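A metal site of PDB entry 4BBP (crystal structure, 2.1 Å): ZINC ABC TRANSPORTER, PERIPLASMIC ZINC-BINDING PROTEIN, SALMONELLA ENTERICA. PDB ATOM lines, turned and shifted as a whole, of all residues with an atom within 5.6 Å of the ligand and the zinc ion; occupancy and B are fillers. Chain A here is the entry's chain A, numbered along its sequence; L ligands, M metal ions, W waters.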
ATOM      1  N   LEU A   7     -31.346   5.519  16.968  1.00  0.00           N
ATOM      2  CA  LEU A   7     -30.076   5.822  16.325  1.00  0.00           C
ATOM      3  C   LEU A   7     -30.312   6.021  14.838  1.00  0.00           C
ATOM      4  O   LEU A   7     -31.245   5.464  14.272  1.00  0.00           O
ATOM      5  CB  LEU A   7     -29.087   4.668  16.546  1.00  0.00           C
ATOM      6  CG  LEU A   7     -28.675   4.338  17.992  1.00  0.00           C
ATOM      7  CD1 LEU A   7     -28.107   2.927  18.130  1.00  0.00           C
ATOM      8  CD2 LEU A   7     -27.681   5.386  18.555  1.00  0.00           C
ATOM      9  N   LEU A  28     -31.632  10.928  19.047  1.00  0.00           N
ATOM     10  CA  LEU A  28     -30.404  11.542  19.540  1.00  0.00           C
ATOM     11  C   LEU A  28     -29.467  11.997  18.410  1.00  0.00           C
ATOM     12  O   LEU A  28     -29.417  11.390  17.351  1.00  0.00           O
ATOM     13  CB  LEU A  28     -29.683  10.546  20.476  1.00  0.00           C
ATOM     14  CG  LEU A  28     -29.029   9.232  19.996  1.00  0.00           C
ATOM     15  CD1 LEU A  28     -29.243   8.890  18.527  1.00  0.00           C
ATOM     16  CD2 LEU A  28     -27.545   9.149  20.339  1.00  0.00           C
ATOM     17  N   ASP A  30     -25.826  12.421  16.597  1.00  0.00           N
ATOM     18  CA  ASP A  30     -24.823  11.384  16.378  1.00  0.00           C
ATOM     19  C   ASP A  30     -23.744  11.339  17.466  1.00  0.00           C
ATOM     20  O   ASP A  30     -23.290  10.251  17.860  1.00  0.00           O
ATOM     21  CB  ASP A  30     -24.193  11.533  14.995  1.00  0.00           C
ATOM     22  CG  ASP A  30     -25.185  11.276  13.874  1.00  0.00           C
ATOM     23  OD1 ASP A  30     -26.112  10.459  14.046  1.00  0.00           O
ATOM     24  OD2 ASP A  30     -25.035  11.900  12.807  1.00  0.00           O
ATOM     25  N   GLY A  31     -23.350  12.500  17.965  1.00  0.00           N
ATOM     26  CA  GLY A  31     -22.264  12.609  18.933  1.00  0.00           C
ATOM     27  C   GLY A  31     -22.494  11.970  20.291  1.00  0.00           C
ATOM     28  O   GLY A  31     -21.565  11.868  21.096  1.00  0.00           O
ATOM     29  N   ALA A  32     -23.733  11.546  20.554  1.00  0.00           N
ATOM     30  CA  ALA A  32     -24.083  10.942  21.822  1.00  0.00           C
ATOM     31  C   ALA A  32     -23.550   9.498  21.916  1.00  0.00           C
ATOM     32  O   ALA A  32     -22.871   9.022  21.005  1.00  0.00           O
ATOM     33  CB  ALA A  32     -25.580  10.994  22.026  1.00  0.00           C
ATOM     34  N   SER A  33     -23.854   8.836  23.042  1.00  0.00           N
ATOM     35  CA  SER A  33     -23.434   7.441  23.306  1.00  0.00           C
ATOM     36  C   SER A  33     -24.486   6.657  24.113  1.00  0.00           C
ATOM     37  O   SER A  33     -25.677   6.988  24.068  1.00  0.00           O
ATOM     38  CB  SER A  33     -22.065   7.406  24.000  1.00  0.00           C
ATOM     39  OG  SER A  33     -22.193   7.770  25.373  1.00  0.00           O
ATOM     40  N   GLU A  34     -24.045   5.639  24.868  1.00  0.00           N
ATOM     41  CA  GLU A  34     -24.944   4.656  25.499  1.00  0.00           C
ATOM     42  C   GLU A  34     -25.075   4.679  27.042  1.00  0.00           C
ATOM     43  O   GLU A  34     -26.145   4.341  27.575  1.00  0.00           O
ATOM     44  CB  GLU A  34     -24.590   3.241  25.036  1.00  0.00           C
ATOM     45  CG  GLU A  34     -23.407   2.577  25.774  1.00  0.00           C
ATOM     46  CD  GLU A  34     -23.811   1.614  26.906  1.00  0.00           C
ATOM     47  OE1 GLU A  34     -24.877   0.962  26.812  1.00  0.00           O
ATOM     48  OE2 GLU A  34     -23.046   1.471  27.881  1.00  0.00           O
ATOM     49  N   MET A  60     -27.699  -2.047  24.432  1.00  0.00           N
ATOM     50  CA  MET A  60     -27.143  -1.008  23.592  1.00  0.00           C
ATOM     51  C   MET A  60     -27.545   0.363  24.173  1.00  0.00           C
ATOM     52  O   MET A  60     -26.776   0.967  24.895  1.00  0.00           O
ATOM     53  CB  MET A  60     -27.549  -1.241  22.117  1.00  0.00           C
ATOM     54  CG  MET A  60     -27.084  -0.222  21.086  1.00  0.00           C
ATOM     55  SD  MET A  60     -25.335   0.258  21.078  1.00  0.00           S
ATOM     56  CE  MET A  60     -24.487  -1.164  20.433  1.00  0.00           C
ATOM     57  N   PHE A  63     -29.524   3.722  28.335  1.00  0.00           N
ATOM     58  CA  PHE A  63     -30.108   4.966  28.811  1.00  0.00           C
ATOM     59  C   PHE A  63     -31.614   5.113  28.547  1.00  0.00           C
ATOM     60  O   PHE A  63     -32.263   5.954  29.163  1.00  0.00           O
ATOM     61  CB  PHE A  63     -29.357   6.169  28.203  1.00  0.00           C
ATOM     62  CG  PHE A  63     -29.464   6.257  26.699  1.00  0.00           C
ATOM     63  CD1 PHE A  63     -30.543   6.889  26.093  1.00  0.00           C
ATOM     64  CD2 PHE A  63     -28.474   5.718  25.880  1.00  0.00           C
ATOM     65  CE1 PHE A  63     -30.648   6.974  24.709  1.00  0.00           C
ATOM     66  CE2 PHE A  63     -28.579   5.802  24.487  1.00  0.00           C
ATOM     67  CZ  PHE A  63     -29.675   6.426  23.913  1.00  0.00           C
ATOM     68  N   HIS A 114     -21.808  -0.383  26.061  1.00  0.00           N
ATOM     69  CA  HIS A 114     -22.508  -1.363  25.232  1.00  0.00           C
ATOM     70  C   HIS A 114     -21.553  -2.401  24.645  1.00  0.00           C
ATOM     71  O   HIS A 114     -21.980  -3.313  23.934  1.00  0.00           O
ATOM     72  CB  HIS A 114     -23.289  -0.667  24.107  1.00  0.00           C
ATOM     73  CG  HIS A 114     -22.436   0.086  23.131  1.00  0.00           C
ATOM     74  ND1 HIS A 114     -22.204   1.435  23.234  1.00  0.00           N
ATOM     75  CD2 HIS A 114     -21.778  -0.321  22.017  1.00  0.00           C
ATOM     76  CE1 HIS A 114     -21.434   1.826  22.236  1.00  0.00           C
ATOM     77  NE2 HIS A 114     -21.171   0.785  21.480  1.00  0.00           N
ATOM     78  N   HIS A 115     -20.256  -2.237  24.933  1.00  0.00           N
ATOM     79  CA  HIS A 115     -19.229  -3.158  24.474  1.00  0.00           C
ATOM     80  C   HIS A 115     -18.917  -4.220  25.526  1.00  0.00           C
ATOM     81  O   HIS A 115     -18.204  -5.193  25.233  1.00  0.00           O
ATOM     82  CB  HIS A 115     -17.952  -2.400  24.087  1.00  0.00           C
ATOM     83  CG  HIS A 115     -18.040  -1.731  22.761  1.00  0.00           C
ATOM     84  ND1 HIS A 115     -17.670  -2.353  21.588  1.00  0.00           N
ATOM     85  CD2 HIS A 115     -18.470  -0.491  22.406  1.00  0.00           C
ATOM     86  CE1 HIS A 115     -17.857  -1.528  20.576  1.00  0.00           C
ATOM     87  NE2 HIS A 115     -18.351  -0.394  21.039  1.00  0.00           N
ATOM     88  N   HIS A 122     -24.071  -3.814  17.675  1.00  0.00           N
ATOM     89  CA  HIS A 122     -24.117  -2.853  16.570  1.00  0.00           C
ATOM     90  C   HIS A 122     -24.891  -3.481  15.416  1.00  0.00           C
ATOM     91  O   HIS A 122     -24.341  -3.677  14.323  1.00  0.00           O
ATOM     92  CB  HIS A 122     -22.727  -2.419  16.109  1.00  0.00           C
ATOM     93  CG  HIS A 122     -21.827  -1.993  17.220  1.00  0.00           C
ATOM     94  ND1 HIS A 122     -21.140  -2.898  18.013  1.00  0.00           N
ATOM     95  CD2 HIS A 122     -21.506  -0.764  17.693  1.00  0.00           C
ATOM     96  CE1 HIS A 122     -20.442  -2.243  18.922  1.00  0.00           C
ATOM     97  NE2 HIS A 122     -20.632  -0.952  18.740  1.00  0.00           N
ATOM     98  N   TRP A 124     -27.326  -2.744  13.375  1.00  0.00           N
ATOM     99  CA  TRP A 124     -27.688  -2.073  12.127  1.00  0.00           C
ATOM    100  C   TRP A 124     -26.679  -2.328  11.009  1.00  0.00           C
ATOM    101  O   TRP A 124     -26.962  -2.062   9.836  1.00  0.00           O
ATOM    102  CB  TRP A 124     -27.854  -0.559  12.364  1.00  0.00           C
ATOM    103  CG  TRP A 124     -26.632   0.109  12.905  1.00  0.00           C
ATOM    104  CD1 TRP A 124     -25.641   0.716  12.184  1.00  0.00           C
ATOM    105  CD2 TRP A 124     -26.246   0.236  14.287  1.00  0.00           C
ATOM    106  NE1 TRP A 124     -24.669   1.218  13.021  1.00  0.00           N
ATOM    107  CE2 TRP A 124     -25.016   0.946  14.321  1.00  0.00           C
ATOM    108  CE3 TRP A 124     -26.833  -0.163  15.498  1.00  0.00           C
ATOM    109  CZ2 TRP A 124     -24.347   1.255  15.523  1.00  0.00           C
ATOM    110  CZ3 TRP A 124     -26.176   0.136  16.692  1.00  0.00           C
ATOM    111  CH2 TRP A 124     -24.939   0.855  16.694  1.00  0.00           C
ATOM    112  N   HIS A 186     -12.563   0.535  16.677  1.00  0.00           N
ATOM    113  CA  HIS A 186     -13.916   0.285  17.205  1.00  0.00           C
ATOM    114  C   HIS A 186     -14.337  -1.119  16.832  1.00  0.00           C
ATOM    115  O   HIS A 186     -14.380  -1.474  15.648  1.00  0.00           O
ATOM    116  CB  HIS A 186     -14.862   1.330  16.622  1.00  0.00           C
ATOM    117  CG  HIS A 186     -16.238   1.324  17.210  1.00  0.00           C
ATOM    118  ND1 HIS A 186     -17.323   1.862  16.548  1.00  0.00           N
ATOM    119  CD2 HIS A 186     -16.719   0.854  18.383  1.00  0.00           C
ATOM    120  CE1 HIS A 186     -18.402   1.726  17.283  1.00  0.00           C
ATOM    121  NE2 HIS A 186     -18.073   1.108  18.410  1.00  0.00           N
ATOM    122  N   ASP A 187     -14.645  -1.948  17.826  1.00  0.00           N
ATOM    123  CA  ASP A 187     -15.114  -3.307  17.567  1.00  0.00           C
ATOM    124  C   ASP A 187     -16.613  -3.282  17.269  1.00  0.00           C
ATOM    125  O   ASP A 187     -17.440  -3.662  18.112  1.00  0.00           O
ATOM    126  CB  ASP A 187     -14.798  -4.222  18.762  1.00  0.00           C
ATOM    127  CG  ASP A 187     -15.196  -5.670  18.511  1.00  0.00           C
ATOM    128  OD1 ASP A 187     -14.982  -6.160  17.387  1.00  0.00           O
ATOM    129  OD2 ASP A 187     -15.712  -6.314  19.446  1.00  0.00           O
ATOM    130  N   ALA A 188     -16.969  -2.808  16.082  1.00  0.00           N
ATOM    131  CA  ALA A 188     -18.375  -2.646  15.707  1.00  0.00           C
ATOM    132  C   ALA A 188     -18.768  -3.437  14.452  1.00  0.00           C
ATOM    133  O   ALA A 188     -19.880  -3.988  14.387  1.00  0.00           O
ATOM    134  CB  ALA A 188     -18.679  -1.167  15.496  1.00  0.00           C
ATOM    135  N   GLU A 235     -12.759   6.568  12.894  1.00  0.00           N
ATOM    136  CA  GLU A 235     -14.134   7.002  12.721  1.00  0.00           C
ATOM    137  C   GLU A 235     -14.163   8.535  12.741  1.00  0.00           C
ATOM    138  O   GLU A 235     -13.158   9.152  13.116  1.00  0.00           O
ATOM    139  CB  GLU A 235     -15.014   6.385  13.824  1.00  0.00           C
ATOM    140  CG  GLU A 235     -15.020   4.870  13.767  1.00  0.00           C
ATOM    141  CD  GLU A 235     -16.097   4.229  14.619  1.00  0.00           C
ATOM    142  OE1 GLU A 235     -16.537   4.841  15.608  1.00  0.00           O
ATOM    143  OE2 GLU A 235     -16.492   3.098  14.299  1.00  0.00           O
ATOM    144  N   PRO A 236     -15.281   9.167  12.330  1.00  0.00           N
ATOM    145  CA  PRO A 236     -15.290  10.629  12.150  1.00  0.00           C
ATOM    146  C   PRO A 236     -14.911  11.459  13.374  1.00  0.00           C
ATOM    147  O   PRO A 236     -14.395  12.545  13.220  1.00  0.00           O
ATOM    148  CB  PRO A 236     -16.742  10.919  11.732  1.00  0.00           C
ATOM    149  CG  PRO A 236     -17.175   9.638  11.052  1.00  0.00           C
ATOM    150  CD  PRO A 236     -16.563   8.556  11.903  1.00  0.00           C
ATOM    151  N   GLN A 237     -15.169  10.941  14.567  1.00  0.00           N
ATOM    152  CA  GLN A 237     -14.939  11.690  15.801  1.00  0.00           C
ATOM    153  C   GLN A 237     -13.472  11.695  16.272  1.00  0.00           C
ATOM    154  O   GLN A 237     -13.125  12.447  17.191  1.00  0.00           O
ATOM    155  CB  GLN A 237     -15.879  11.204  16.913  1.00  0.00           C
ATOM    156  CG  GLN A 237     -15.532   9.828  17.536  1.00  0.00           C
ATOM    157  CD  GLN A 237     -16.049   8.639  16.719  1.00  0.00           C
ATOM    158  OE1 GLN A 237     -16.029   7.504  17.202  1.00  0.00           O
ATOM    159  NE2 GLN A 237     -16.528   8.901  15.506  1.00  0.00           N
ATOM    160  N   ASP A 258     -17.627   5.314   8.930  1.00  0.00           N
ATOM    161  CA  ASP A 258     -18.688   5.978   9.649  1.00  0.00           C
ATOM    162  C   ASP A 258     -19.841   5.001   9.873  1.00  0.00           C
ATOM    163  O   ASP A 258     -20.649   4.778   8.973  1.00  0.00           O
ATOM    164  CB  ASP A 258     -19.148   7.236   8.903  1.00  0.00           C
ATOM    165  CG  ASP A 258     -20.259   7.980   9.633  1.00  0.00           C
ATOM    166  OD1 ASP A 258     -20.611   7.610  10.777  1.00  0.00           O
ATOM    167  OD2 ASP A 258     -20.802   8.937   9.053  1.00  0.00           O
ATOM    168  N   PRO A 259     -19.915   4.416  11.091  1.00  0.00           N
ATOM    169  CA  PRO A 259     -20.889   3.355  11.382  1.00  0.00           C
ATOM    170  C   PRO A 259     -22.317   3.897  11.572  1.00  0.00           C
ATOM    171  O   PRO A 259     -23.256   3.109  11.733  1.00  0.00           O
ATOM    172  CB  PRO A 259     -20.370   2.778  12.698  1.00  0.00           C
ATOM    173  CG  PRO A 259     -19.744   3.951  13.394  1.00  0.00           C
ATOM    174  CD  PRO A 259     -19.136   4.786  12.288  1.00  0.00           C
ATOM    175  N   LEU A 260     -22.461   5.217  11.545  1.00  0.00           N
ATOM    176  CA  LEU A 260     -23.773   5.839  11.698  1.00  0.00           C
ATOM    177  C   LEU A 260     -24.288   6.538  10.425  1.00  0.00           C
ATOM    178  O   LEU A 260     -25.406   7.021  10.404  1.00  0.00           O
ATOM    179  CB  LEU A 260     -23.781   6.824  12.873  1.00  0.00           C
ATOM    180  CG  LEU A 260     -23.502   6.321  14.291  1.00  0.00           C
ATOM    181  CD1 LEU A 260     -23.289   7.542  15.169  1.00  0.00           C
ATOM    182  CD2 LEU A 260     -24.638   5.454  14.860  1.00  0.00           C
ATOM    183  N   THR A 262     -23.562   9.415   9.295  1.00  0.00           N
ATOM    184  CA  THR A 262     -23.888  10.779   9.738  1.00  0.00           C
ATOM    185  C   THR A 262     -24.308  11.747   8.601  1.00  0.00           C
ATOM    186  O   THR A 262     -25.172  12.604   8.805  1.00  0.00           O
ATOM    187  CB  THR A 262     -22.692  11.429  10.504  1.00  0.00           C
ATOM    188  OG1 THR A 262     -21.522  11.430   9.666  1.00  0.00           O
ATOM    189  CG2 THR A 262     -22.396  10.659  11.794  1.00  0.00           C
HETATM  190 CL1  LIG L   1     -19.940   8.620  13.451  1.00  0.00          CL
HETATM  191  C1  LIG L   1     -19.768   9.321  15.096  1.00  0.00           C
HETATM  192  C2  LIG L   1     -19.882  10.701  15.264  1.00  0.00           C
HETATM  193  C3  LIG L   1     -19.749  11.262  16.539  1.00  0.00           C
HETATM  194  C4  LIG L   1     -19.513  10.431  17.637  1.00  0.00           C
HETATM  195  C5  LIG L   1     -19.409   9.051  17.470  1.00  0.00           C
HETATM  196  C6  LIG L   1     -19.543   8.480  16.196  1.00  0.00           C
HETATM  197  C7  LIG L   1     -19.425   6.977  15.974  1.00  0.00           C
HETATM  198  N1  LIG L   1     -20.028   6.149  17.029  1.00  0.00           N
HETATM  199  C8  LIG L   1     -19.450   5.070  17.562  1.00  0.00           C
HETATM  200  C9  LIG L   1     -21.233   6.314  17.619  1.00  0.00           C
HETATM  201  C10 LIG L   1     -21.456   5.322  18.563  1.00  0.00           C
HETATM  202  C11 LIG L   1     -20.316   4.535  18.507  1.00  0.00           C
HETATM  203  C12 LIG L   1     -20.104   3.351  19.375  1.00  0.00           C
HETATM  204  N2  LIG L   1     -19.254   3.532  20.394  1.00  0.00           N
HETATM  205  O1  LIG L   1     -18.593   2.489  21.037  1.00  0.00           O
HETATM  206  O2  LIG L   1     -20.710   2.294  19.154  1.00  0.00           O
HETATM  207  C13 LIG L   1     -22.597   5.180  19.385  1.00  0.00           C
HETATM  208  C14 LIG L   1     -22.711   4.128  20.310  1.00  0.00           C
HETATM  209  C15 LIG L   1     -23.844   3.984  21.111  1.00  0.00           C
HETATM  210  C16 LIG L   1     -24.882   4.904  20.998  1.00  0.00           C
HETATM  211  C17 LIG L   1     -24.776   5.956  20.083  1.00  0.00           C
HETATM  212  C18 LIG L   1     -23.643   6.090  19.283  1.00  0.00           C
HETATM  213 ZN    ZN M   1     -19.679   0.702  19.788  1.00  0.00          ZN
HETATM  214  O   HOH W   1     -25.440   8.372  17.966  1.00  0.00           O
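OE2 of Glu 235 is in hydrogen-bond range of ND1 of His 186 (2.7 Å).
The backbone carbonyl oxygen (O) of Pro 259 sits at hydrogen-bond distance from the indole nitrogen (NE1) of Trp 124, 2.7 Å away.
OE1 of Gln 237 lies close to OE1 of Glu 235 (3.1 Å).
OE2 of Glu 34 is in hydrogen-bond range of N of His 114 (2.9 Å).
The side-chain carboxylate (OD1) of Asp 258 sits close to the backbone NH (N) of Leu 260, at 3.1 Å.
OD2 of Asp 258 is in hydrogen-bond range of OG1 of Thr 262 (2.7 Å).
Within 4 Å of the zinc ion: His 114, His 115, His 122 and His 186.
The zinc ion is bound by O2 of the ligand (2.0 Å), NE2 of His 115 (2.1 Å), NE2 of His 186 (2.2 Å), NE2 of His 122 (2.2 Å), NE2 of His 114 (2.3 Å) and O1 of the ligand (2.4 Å).
Merely in contact with the ligand: Asp 258 (2.9 Å), Gln 237 (3.1 Å), Leu 7 (3.3 Å), Leu 260 (3.4 Å), Ala 32 (3.5 Å), Glu 235 (3.5 Å), Ser 33 (3.6 Å), Thr 262 (3.6 Å), Pro 236 (3.7 Å), Gly 31 (3.7 Å), Asp 30 (3.8 Å) and Pro 259 (3.99 Å).
Hydrophobic or aromatic side chains within 4 Å of the ligand: Leu 7, His 114, His 115, His 122, His 186, Pro 236, Pro 259 and Leu 260.
Within 4 Å of the ligand: Leu 7, Asp 30, Gly 31, Ala 32, Ser 33, His 114, His 115, His 122, His 186, Glu 235, Pro 236, Gln 237, Asp 258, Pro 259, Leu 260 and Thr 262.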
